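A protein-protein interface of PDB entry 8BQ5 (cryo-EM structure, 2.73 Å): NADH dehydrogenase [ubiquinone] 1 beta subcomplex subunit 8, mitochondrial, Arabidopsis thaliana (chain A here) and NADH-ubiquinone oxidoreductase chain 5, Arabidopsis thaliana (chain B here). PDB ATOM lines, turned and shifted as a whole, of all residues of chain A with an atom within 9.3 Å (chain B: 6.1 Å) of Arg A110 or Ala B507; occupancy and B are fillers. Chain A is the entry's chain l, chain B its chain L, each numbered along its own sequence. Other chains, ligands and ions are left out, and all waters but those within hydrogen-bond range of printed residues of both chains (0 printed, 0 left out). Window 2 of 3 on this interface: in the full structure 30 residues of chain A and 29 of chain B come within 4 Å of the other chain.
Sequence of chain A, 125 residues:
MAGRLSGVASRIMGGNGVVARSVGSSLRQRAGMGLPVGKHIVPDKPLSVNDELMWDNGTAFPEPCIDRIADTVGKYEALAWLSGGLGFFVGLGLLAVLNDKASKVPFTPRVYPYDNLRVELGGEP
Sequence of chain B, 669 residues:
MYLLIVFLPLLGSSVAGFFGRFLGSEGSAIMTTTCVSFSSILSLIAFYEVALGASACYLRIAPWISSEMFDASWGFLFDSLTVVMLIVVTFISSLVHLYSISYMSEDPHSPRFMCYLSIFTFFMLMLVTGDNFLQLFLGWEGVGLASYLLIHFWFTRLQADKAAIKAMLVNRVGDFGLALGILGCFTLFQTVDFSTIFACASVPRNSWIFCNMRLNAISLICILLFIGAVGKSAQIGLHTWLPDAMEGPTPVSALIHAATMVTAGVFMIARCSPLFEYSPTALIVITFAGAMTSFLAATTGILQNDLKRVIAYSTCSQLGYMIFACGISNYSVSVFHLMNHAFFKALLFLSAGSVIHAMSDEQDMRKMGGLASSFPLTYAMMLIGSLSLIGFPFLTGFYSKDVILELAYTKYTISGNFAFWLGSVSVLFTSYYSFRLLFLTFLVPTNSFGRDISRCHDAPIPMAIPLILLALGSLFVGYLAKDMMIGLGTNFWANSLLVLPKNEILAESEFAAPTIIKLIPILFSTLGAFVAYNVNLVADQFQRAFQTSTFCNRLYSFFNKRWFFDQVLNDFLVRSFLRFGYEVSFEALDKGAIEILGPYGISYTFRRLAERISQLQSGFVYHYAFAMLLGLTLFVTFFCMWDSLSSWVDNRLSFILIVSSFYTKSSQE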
ATOM      1  N   VAL A 105     -21.344 -26.211  11.527  1.00  0.00           N
ATOM      2  CA  VAL A 105     -22.080 -25.940  12.801  1.00  0.00           C
ATOM      3  C   VAL A 105     -23.569 -25.764  12.485  1.00  0.00           C
ATOM      4  O   VAL A 105     -23.886 -25.010  11.548  1.00  0.00           O
ATOM      5  CB  VAL A 105     -21.488 -24.729  13.550  1.00  0.00           C
ATOM      6  CG1 VAL A 105     -21.253 -23.529  12.645  1.00  0.00           C
ATOM      7  CG2 VAL A 105     -22.293 -24.342  14.779  1.00  0.00           C
ATOM      8  N   PHE A 107     -26.073 -24.324  14.210  1.00  0.00           N
ATOM      9  CA  PHE A 107     -26.767 -23.203  14.822  1.00  0.00           C
ATOM     10  C   PHE A 107     -25.919 -21.947  14.696  1.00  0.00           C
ATOM     11  O   PHE A 107     -24.691 -22.012  14.618  1.00  0.00           O
ATOM     12  CB  PHE A 107     -27.091 -23.492  16.297  1.00  0.00           C
ATOM     13  CG  PHE A 107     -25.942 -24.082  17.069  1.00  0.00           C
ATOM     14  CD1 PHE A 107     -24.914 -23.279  17.535  1.00  0.00           C
ATOM     15  CD2 PHE A 107     -25.887 -25.444  17.322  1.00  0.00           C
ATOM     16  CE1 PHE A 107     -23.857 -23.818  18.244  1.00  0.00           C
ATOM     17  CE2 PHE A 107     -24.830 -25.990  18.030  1.00  0.00           C
ATOM     18  CZ  PHE A 107     -23.814 -25.175  18.489  1.00  0.00           C
ATOM     19  N   THR A 108     -26.593 -20.799  14.674  1.00  0.00           N
ATOM     20  CA  THR A 108     -25.911 -19.521  14.612  1.00  0.00           C
ATOM     21  C   THR A 108     -25.257 -19.206  15.955  1.00  0.00           C
ATOM     22  O   THR A 108     -25.647 -19.752  16.988  1.00  0.00           O
ATOM     23  CB  THR A 108     -26.891 -18.411  14.243  1.00  0.00           C
ATOM     24  OG1 THR A 108     -27.885 -18.296  15.267  1.00  0.00           O
ATOM     25  CG2 THR A 108     -27.570 -18.713  12.924  1.00  0.00           C
ATOM     26  N   PRO A 109     -24.250 -18.334  15.966  1.00  0.00           N
ATOM     27  CA  PRO A 109     -23.682 -17.896  17.245  1.00  0.00           C
ATOM     28  C   PRO A 109     -24.706 -17.140  18.077  1.00  0.00           C
ATOM     29  O   PRO A 109     -25.576 -16.442  17.552  1.00  0.00           O
ATOM     30  CB  PRO A 109     -22.518 -16.986  16.833  1.00  0.00           C
ATOM     31  CG  PRO A 109     -22.233 -17.324  15.412  1.00  0.00           C
ATOM     32  CD  PRO A 109     -23.529 -17.763  14.815  1.00  0.00           C
ATOM     33  N   ARG A 110     -24.590 -17.295  19.394  1.00  0.00           N
ATOM     34  CA  ARG A 110     -25.465 -16.586  20.314  1.00  0.00           C
ATOM     35  C   ARG A 110     -25.307 -15.079  20.145  1.00  0.00           C
ATOM     36  O   ARG A 110     -24.210 -14.569  19.899  1.00  0.00           O
ATOM     37  CB  ARG A 110     -25.153 -16.968  21.763  1.00  0.00           C
ATOM     38  CG  ARG A 110     -25.345 -18.435  22.123  1.00  0.00           C
ATOM     39  CD  ARG A 110     -25.164 -18.625  23.625  1.00  0.00           C
ATOM     40  NE  ARG A 110     -24.923 -20.013  24.004  1.00  0.00           N
ATOM     41  CZ  ARG A 110     -25.360 -20.568  25.127  1.00  0.00           C
ATOM     42  NH1 ARG A 110     -26.056 -19.878  26.014  1.00  0.00           N
ATOM     43  NH2 ARG A 110     -25.085 -21.847  25.368  1.00  0.00           N
ATOM     44  N   VAL A 111     -26.421 -14.364  20.269  1.00  0.00           N
ATOM     45  CA  VAL A 111     -26.419 -12.906  20.282  1.00  0.00           C
ATOM     46  C   VAL A 111     -27.078 -12.481  21.586  1.00  0.00           C
ATOM     47  O   VAL A 111     -28.248 -12.803  21.826  1.00  0.00           O
ATOM     48  CB  VAL A 111     -27.152 -12.297  19.078  1.00  0.00           C
ATOM     49  CG1 VAL A 111     -27.409 -10.816  19.309  1.00  0.00           C
ATOM     50  CG2 VAL A 111     -26.350 -12.510  17.808  1.00  0.00           C
ATOM     51  N   TYR A 112     -26.340 -11.767  22.425  1.00  0.00           N
ATOM     52  CA  TYR A 112     -26.829 -11.409  23.744  1.00  0.00           C
ATOM     53  C   TYR A 112     -27.423 -10.003  23.744  1.00  0.00           C
ATOM     54  O   TYR A 112     -27.007  -9.139  22.971  1.00  0.00           O
ATOM     55  CB  TYR A 112     -25.697 -11.519  24.761  1.00  0.00           C
ATOM     56  CG  TYR A 112     -25.434 -12.943  25.203  1.00  0.00           C
ATOM     57  CD1 TYR A 112     -24.719 -13.821  24.398  1.00  0.00           C
ATOM     58  CD2 TYR A 112     -25.909 -13.409  26.420  1.00  0.00           C
ATOM     59  CE1 TYR A 112     -24.484 -15.126  24.798  1.00  0.00           C
ATOM     60  CE2 TYR A 112     -25.677 -14.707  26.829  1.00  0.00           C
ATOM     61  CZ  TYR A 112     -24.966 -15.560  26.016  1.00  0.00           C
ATOM     62  OH  TYR A 112     -24.738 -16.853  26.424  1.00  0.00           O
ATOM     63  N   PRO A 113     -28.417  -9.754  24.601  1.00  0.00           N
ATOM     64  CA  PRO A 113     -29.043  -8.425  24.644  1.00  0.00           C
ATOM     65  C   PRO A 113     -28.149  -7.356  25.252  1.00  0.00           C
ATOM     66  O   PRO A 113     -27.117  -7.663  25.857  1.00  0.00           O
ATOM     67  CB  PRO A 113     -30.295  -8.657  25.499  1.00  0.00           C
ATOM     68  CG  PRO A 113     -29.957  -9.842  26.335  1.00  0.00           C
ATOM     69  CD  PRO A 113     -29.115 -10.721  25.465  1.00  0.00           C
ATOM     70  N   ASN A 116     -24.705  -7.071  23.243  1.00  0.00           N
ATOM     71  CA  ASN A 116     -23.954  -8.289  23.551  1.00  0.00           C
ATOM     72  C   ASN A 116     -23.227  -8.172  24.889  1.00  0.00           C
ATOM     73  O   ASN A 116     -22.067  -8.567  25.021  1.00  0.00           O
ATOM     74  CB  ASN A 116     -22.972  -8.635  22.429  1.00  0.00           C
ATOM     75  CG  ASN A 116     -22.395 -10.024  22.574  1.00  0.00           C
ATOM     76  OD1 ASN A 116     -23.050 -10.929  23.093  1.00  0.00           O
ATOM     77  ND2 ASN A 116     -21.166 -10.206  22.109  1.00  0.00           N
ATOM     78  N   LEU A 117     -23.922  -7.619  25.881  1.00  0.00           N
ATOM     79  CA  LEU A 117     -23.389  -7.442  27.232  1.00  0.00           C
ATOM     80  C   LEU A 117     -22.075  -6.666  27.213  1.00  0.00           C
ATOM     81  O   LEU A 117     -21.075  -7.074  27.804  1.00  0.00           O
ATOM     82  CB  LEU A 117     -23.223  -8.790  27.934  1.00  0.00           C
ATOM     83  CG  LEU A 117     -24.476  -9.660  28.015  1.00  0.00           C
ATOM     84  CD1 LEU A 117     -24.125 -11.064  28.476  1.00  0.00           C
ATOM     85  CD2 LEU A 117     -25.489  -9.024  28.949  1.00  0.00           C
ATOM     86  N   LEU B 488     -28.646 -26.070  34.182  1.00  0.00           N
ATOM     87  CA  LEU B 488     -28.683 -24.928  33.275  1.00  0.00           C
ATOM     88  C   LEU B 488     -28.959 -23.637  34.030  1.00  0.00           C
ATOM     89  O   LEU B 488     -30.039 -23.455  34.599  1.00  0.00           O
ATOM     90  CB  LEU B 488     -29.749 -25.155  32.201  1.00  0.00           C
ATOM     91  CG  LEU B 488     -29.430 -24.658  30.791  1.00  0.00           C
ATOM     92  CD1 LEU B 488     -28.228 -25.384  30.228  1.00  0.00           C
ATOM     93  CD2 LEU B 488     -30.633 -24.843  29.884  1.00  0.00           C
ATOM     94  N   PRO B 501     -19.624 -15.287  27.726  1.00  0.00           N
ATOM     95  CA  PRO B 501     -20.809 -15.635  26.919  1.00  0.00           C
ATOM     96  C   PRO B 501     -20.477 -16.299  25.594  1.00  0.00           C
ATOM     97  O   PRO B 501     -21.226 -17.170  25.134  1.00  0.00           O
ATOM     98  CB  PRO B 501     -21.496 -14.278  26.724  1.00  0.00           C
ATOM     99  CG  PRO B 501     -21.063 -13.459  27.886  1.00  0.00           C
ATOM    100  CD  PRO B 501     -19.698 -13.927  28.284  1.00  0.00           C
ATOM    101  N   GLU B 504     -20.205 -20.192  26.281  1.00  0.00           N
ATOM    102  CA  GLU B 504     -21.281 -21.015  26.817  1.00  0.00           C
ATOM    103  C   GLU B 504     -21.840 -21.926  25.730  1.00  0.00           C
ATOM    104  O   GLU B 504     -22.329 -21.449  24.701  1.00  0.00           O
ATOM    105  CB  GLU B 504     -22.384 -20.138  27.401  1.00  0.00           C
ATOM    106  CG  GLU B 504     -22.484 -20.193  28.913  1.00  0.00           C
ATOM    107  CD  GLU B 504     -22.876 -21.572  29.416  1.00  0.00           C
ATOM    108  OE1 GLU B 504     -24.089 -21.825  29.576  1.00  0.00           O
ATOM    109  OE2 GLU B 504     -21.974 -22.404  29.654  1.00  0.00           O
ATOM    110  N   ILE B 505     -21.766 -23.239  25.960  1.00  0.00           N
ATOM    111  CA  ILE B 505     -22.281 -24.230  25.025  1.00  0.00           C
ATOM    112  C   ILE B 505     -23.129 -25.295  25.703  1.00  0.00           C
ATOM    113  O   ILE B 505     -23.422 -26.320  25.087  1.00  0.00           O
ATOM    114  CB  ILE B 505     -21.140 -24.895  24.228  1.00  0.00           C
ATOM    115  CG1 ILE B 505     -20.180 -25.619  25.175  1.00  0.00           C
ATOM    116  CG2 ILE B 505     -20.400 -23.861  23.396  1.00  0.00           C
ATOM    117  CD1 ILE B 505     -19.150 -26.479  24.472  1.00  0.00           C
ATOM    118  N   LEU B 506     -23.529 -25.092  26.960  1.00  0.00           N
ATOM    119  CA  LEU B 506     -24.248 -26.135  27.685  1.00  0.00           C
ATOM    120  C   LEU B 506     -25.651 -26.335  27.122  1.00  0.00           C
ATOM    121  O   LEU B 506     -26.101 -27.472  26.940  1.00  0.00           O
ATOM    122  CB  LEU B 506     -24.304 -25.791  29.172  1.00  0.00           C
ATOM    123  CG  LEU B 506     -24.858 -26.870  30.103  1.00  0.00           C
ATOM    124  CD1 LEU B 506     -24.002 -28.121  30.040  1.00  0.00           C
ATOM    125  CD2 LEU B 506     -24.923 -26.341  31.522  1.00  0.00           C
ATOM    126  N   ALA B 507     -26.358 -25.238  26.845  1.00  0.00           N
ATOM    127  CA  ALA B 507     -27.717 -25.343  26.322  1.00  0.00           C
ATOM    128  C   ALA B 507     -27.739 -26.104  25.003  1.00  0.00           C
ATOM    129  O   ALA B 507     -28.513 -27.053  24.831  1.00  0.00           O
ATOM    130  CB  ALA B 507     -28.321 -23.949  26.149  1.00  0.00           C
ATOM    131  N   GLU B 508     -26.875 -25.713  24.064  1.00  0.00           N
ATOM    132  CA  GLU B 508     -26.838 -26.375  22.765  1.00  0.00           C
ATOM    133  C   GLU B 508     -26.440 -27.840  22.883  1.00  0.00           C
ATOM    134  O   GLU B 508     -26.845 -28.659  22.051  1.00  0.00           O
ATOM    135  CB  GLU B 508     -25.883 -25.633  21.834  1.00  0.00           C
ATOM    136  CG  GLU B 508     -26.245 -24.173  21.638  1.00  0.00           C
ATOM    137  CD  GLU B 508     -25.443 -23.244  22.526  1.00  0.00           C
ATOM    138  OE1 GLU B 508     -25.333 -23.526  23.737  1.00  0.00           O
ATOM    139  OE2 GLU B 508     -24.936 -22.225  22.014  1.00  0.00           O
ATOM    140  N   SER B 509     -25.648 -28.192  23.896  1.00  0.00           N
ATOM    141  CA  SER B 509     -25.230 -29.582  24.041  1.00  0.00           C
ATOM    142  C   SER B 509     -26.409 -30.482  24.396  1.00  0.00           C
ATOM    143  O   SER B 509     -26.498 -31.615  23.909  1.00  0.00           O
ATOM    144  CB  SER B 509     -24.121 -29.695  25.089  1.00  0.00           C
ATOM    145  OG  SER B 509     -24.650 -29.932  26.380  1.00  0.00           O
ATOM    146  N   GLU B 510     -27.325 -29.999  25.236  1.00  0.00           N
ATOM    147  CA  GLU B 510     -28.443 -30.818  25.685  1.00  0.00           C
ATOM    148  C   GLU B 510     -29.700 -30.651  24.837  1.00  0.00           C
ATOM    149  O   GLU B 510     -30.691 -31.339  25.098  1.00  0.00           O
ATOM    150  CB  GLU B 510     -28.768 -30.507  27.152  1.00  0.00           C
ATOM    151  CG  GLU B 510     -29.414 -29.146  27.392  1.00  0.00           C
ATOM    152  CD  GLU B 510     -30.096 -29.048  28.748  1.00  0.00           C
ATOM    153  OE1 GLU B 510     -30.759 -30.022  29.161  1.00  0.00           O
ATOM    154  OE2 GLU B 510     -29.965 -27.994  29.404  1.00  0.00           O
ATOM    155  N   PHE B 511     -29.689 -29.773  23.832  1.00  0.00           N
ATOM    156  CA  PHE B 511     -30.896 -29.524  23.052  1.00  0.00           C
ATOM    157  C   PHE B 511     -30.660 -29.682  21.554  1.00  0.00           C
ATOM    158  O   PHE B 511     -31.560 -30.108  20.822  1.00  0.00           O
ATOM    159  CB  PHE B 511     -31.438 -28.123  23.340  1.00  0.00           C
ATOM    160  CG  PHE B 511     -31.894 -27.924  24.756  1.00  0.00           C
ATOM    161  CD1 PHE B 511     -32.654 -28.886  25.398  1.00  0.00           C
ATOM    162  CD2 PHE B 511     -31.572 -26.766  25.442  1.00  0.00           C
ATOM    163  CE1 PHE B 511     -33.075 -28.700  26.698  1.00  0.00           C
ATOM    164  CE2 PHE B 511     -31.992 -26.574  26.742  1.00  0.00           C
ATOM    165  CZ  PHE B 511     -32.745 -27.544  27.370  1.00  0.00           C
ATOM    166  N   ALA B 512     -29.465 -29.330  21.084  1.00  0.00           N
ATOM    167  CA  ALA B 512     -29.149 -29.348  19.662  1.00  0.00           C
ATOM    168  C   ALA B 512     -28.330 -30.563  19.249  1.00  0.00           C
ATOM    169  O   ALA B 512     -27.814 -30.595  18.128  1.00  0.00           O
ATOM    170  CB  ALA B 512     -28.410 -28.067  19.270  1.00  0.00           C
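O of Glu B504 sits at hydrogen-bond distance from NH2 of Arg A110, at 2.9 Å. The guanidinium group (NE) of Arg A110 is in salt-bridge range of the side-chain carboxylate (OE2) of Glu B508, at 3.0 Å.
N of Tyr A112 lies close to OD1 of Asn A116. The guanidinium group of Arg A110 is in hydrogen-bond range of the side-chain hydroxyl of Tyr A112 (3.3 Å). The side-chain hydroxyl (OG) of Ser B509 lies within hydrogen-bond range of the backbone carbonyl oxygen (O) of Leu B506 (2.9 Å).
Among the printed residues, merely in contact across the chains: Arg A110 with Ile B505 (3.6 Å), Tyr A112 with Pro B501 (3.7 Å), Arg A110 with Ala B507 (3.9 Å), Leu A117 with Pro B501 (3.9 Å), Arg A110 with Leu B506 (3.9 Å) and Phe A107 with Glu B508 (3.96 Å).
Of the printed residues of chain B, Phe A107 touches Glu B508 (3.96 Å). Pro A109 touches none of the printed residues of chain B. Arg A110 touches just these residues of chain B: Glu B504, Ile B505, Leu B506, Ala B507 and Glu B508. Printed residues of chain B within 4 Å of Tyr A112: Pro B501 (3.7 Å). Of chain A, only Arg A110 (3.9 Å) comes within 4 Å of Ala B507. Of chain A, only Phe A107 (3.96 Å) and Arg A110 (2.4 Å) come within 4 Å of Glu B508. No residue of chain A comes within 4 Å of Ser B509. Phe B511 touches none of the printed residues of chain A. The nearest residue of chain B that does not touch Arg A110 is Pro B501 (4.5 Å). The nearest printed residue of chain B that does not touch Leu A117 is Glu B504 (9.3 Å).
Of the 11 printed residues of chain B, 6 touch a printed residue of chain A. Printed residues of chain B that touch a printed residue of chain A: Pro B501, Glu B504, Ile B505, Leu B506, Ala B507 and Glu B508. Hydrophobic or aromatic side chains of chain B that line the printed part of chain A: Pro B501 and Ala B507. Among the printed residues, Asp or Glu carboxylates within 4 Å of a Lys or Arg side-chain nitrogen of the other chain: Arg A110 with Glu B508.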
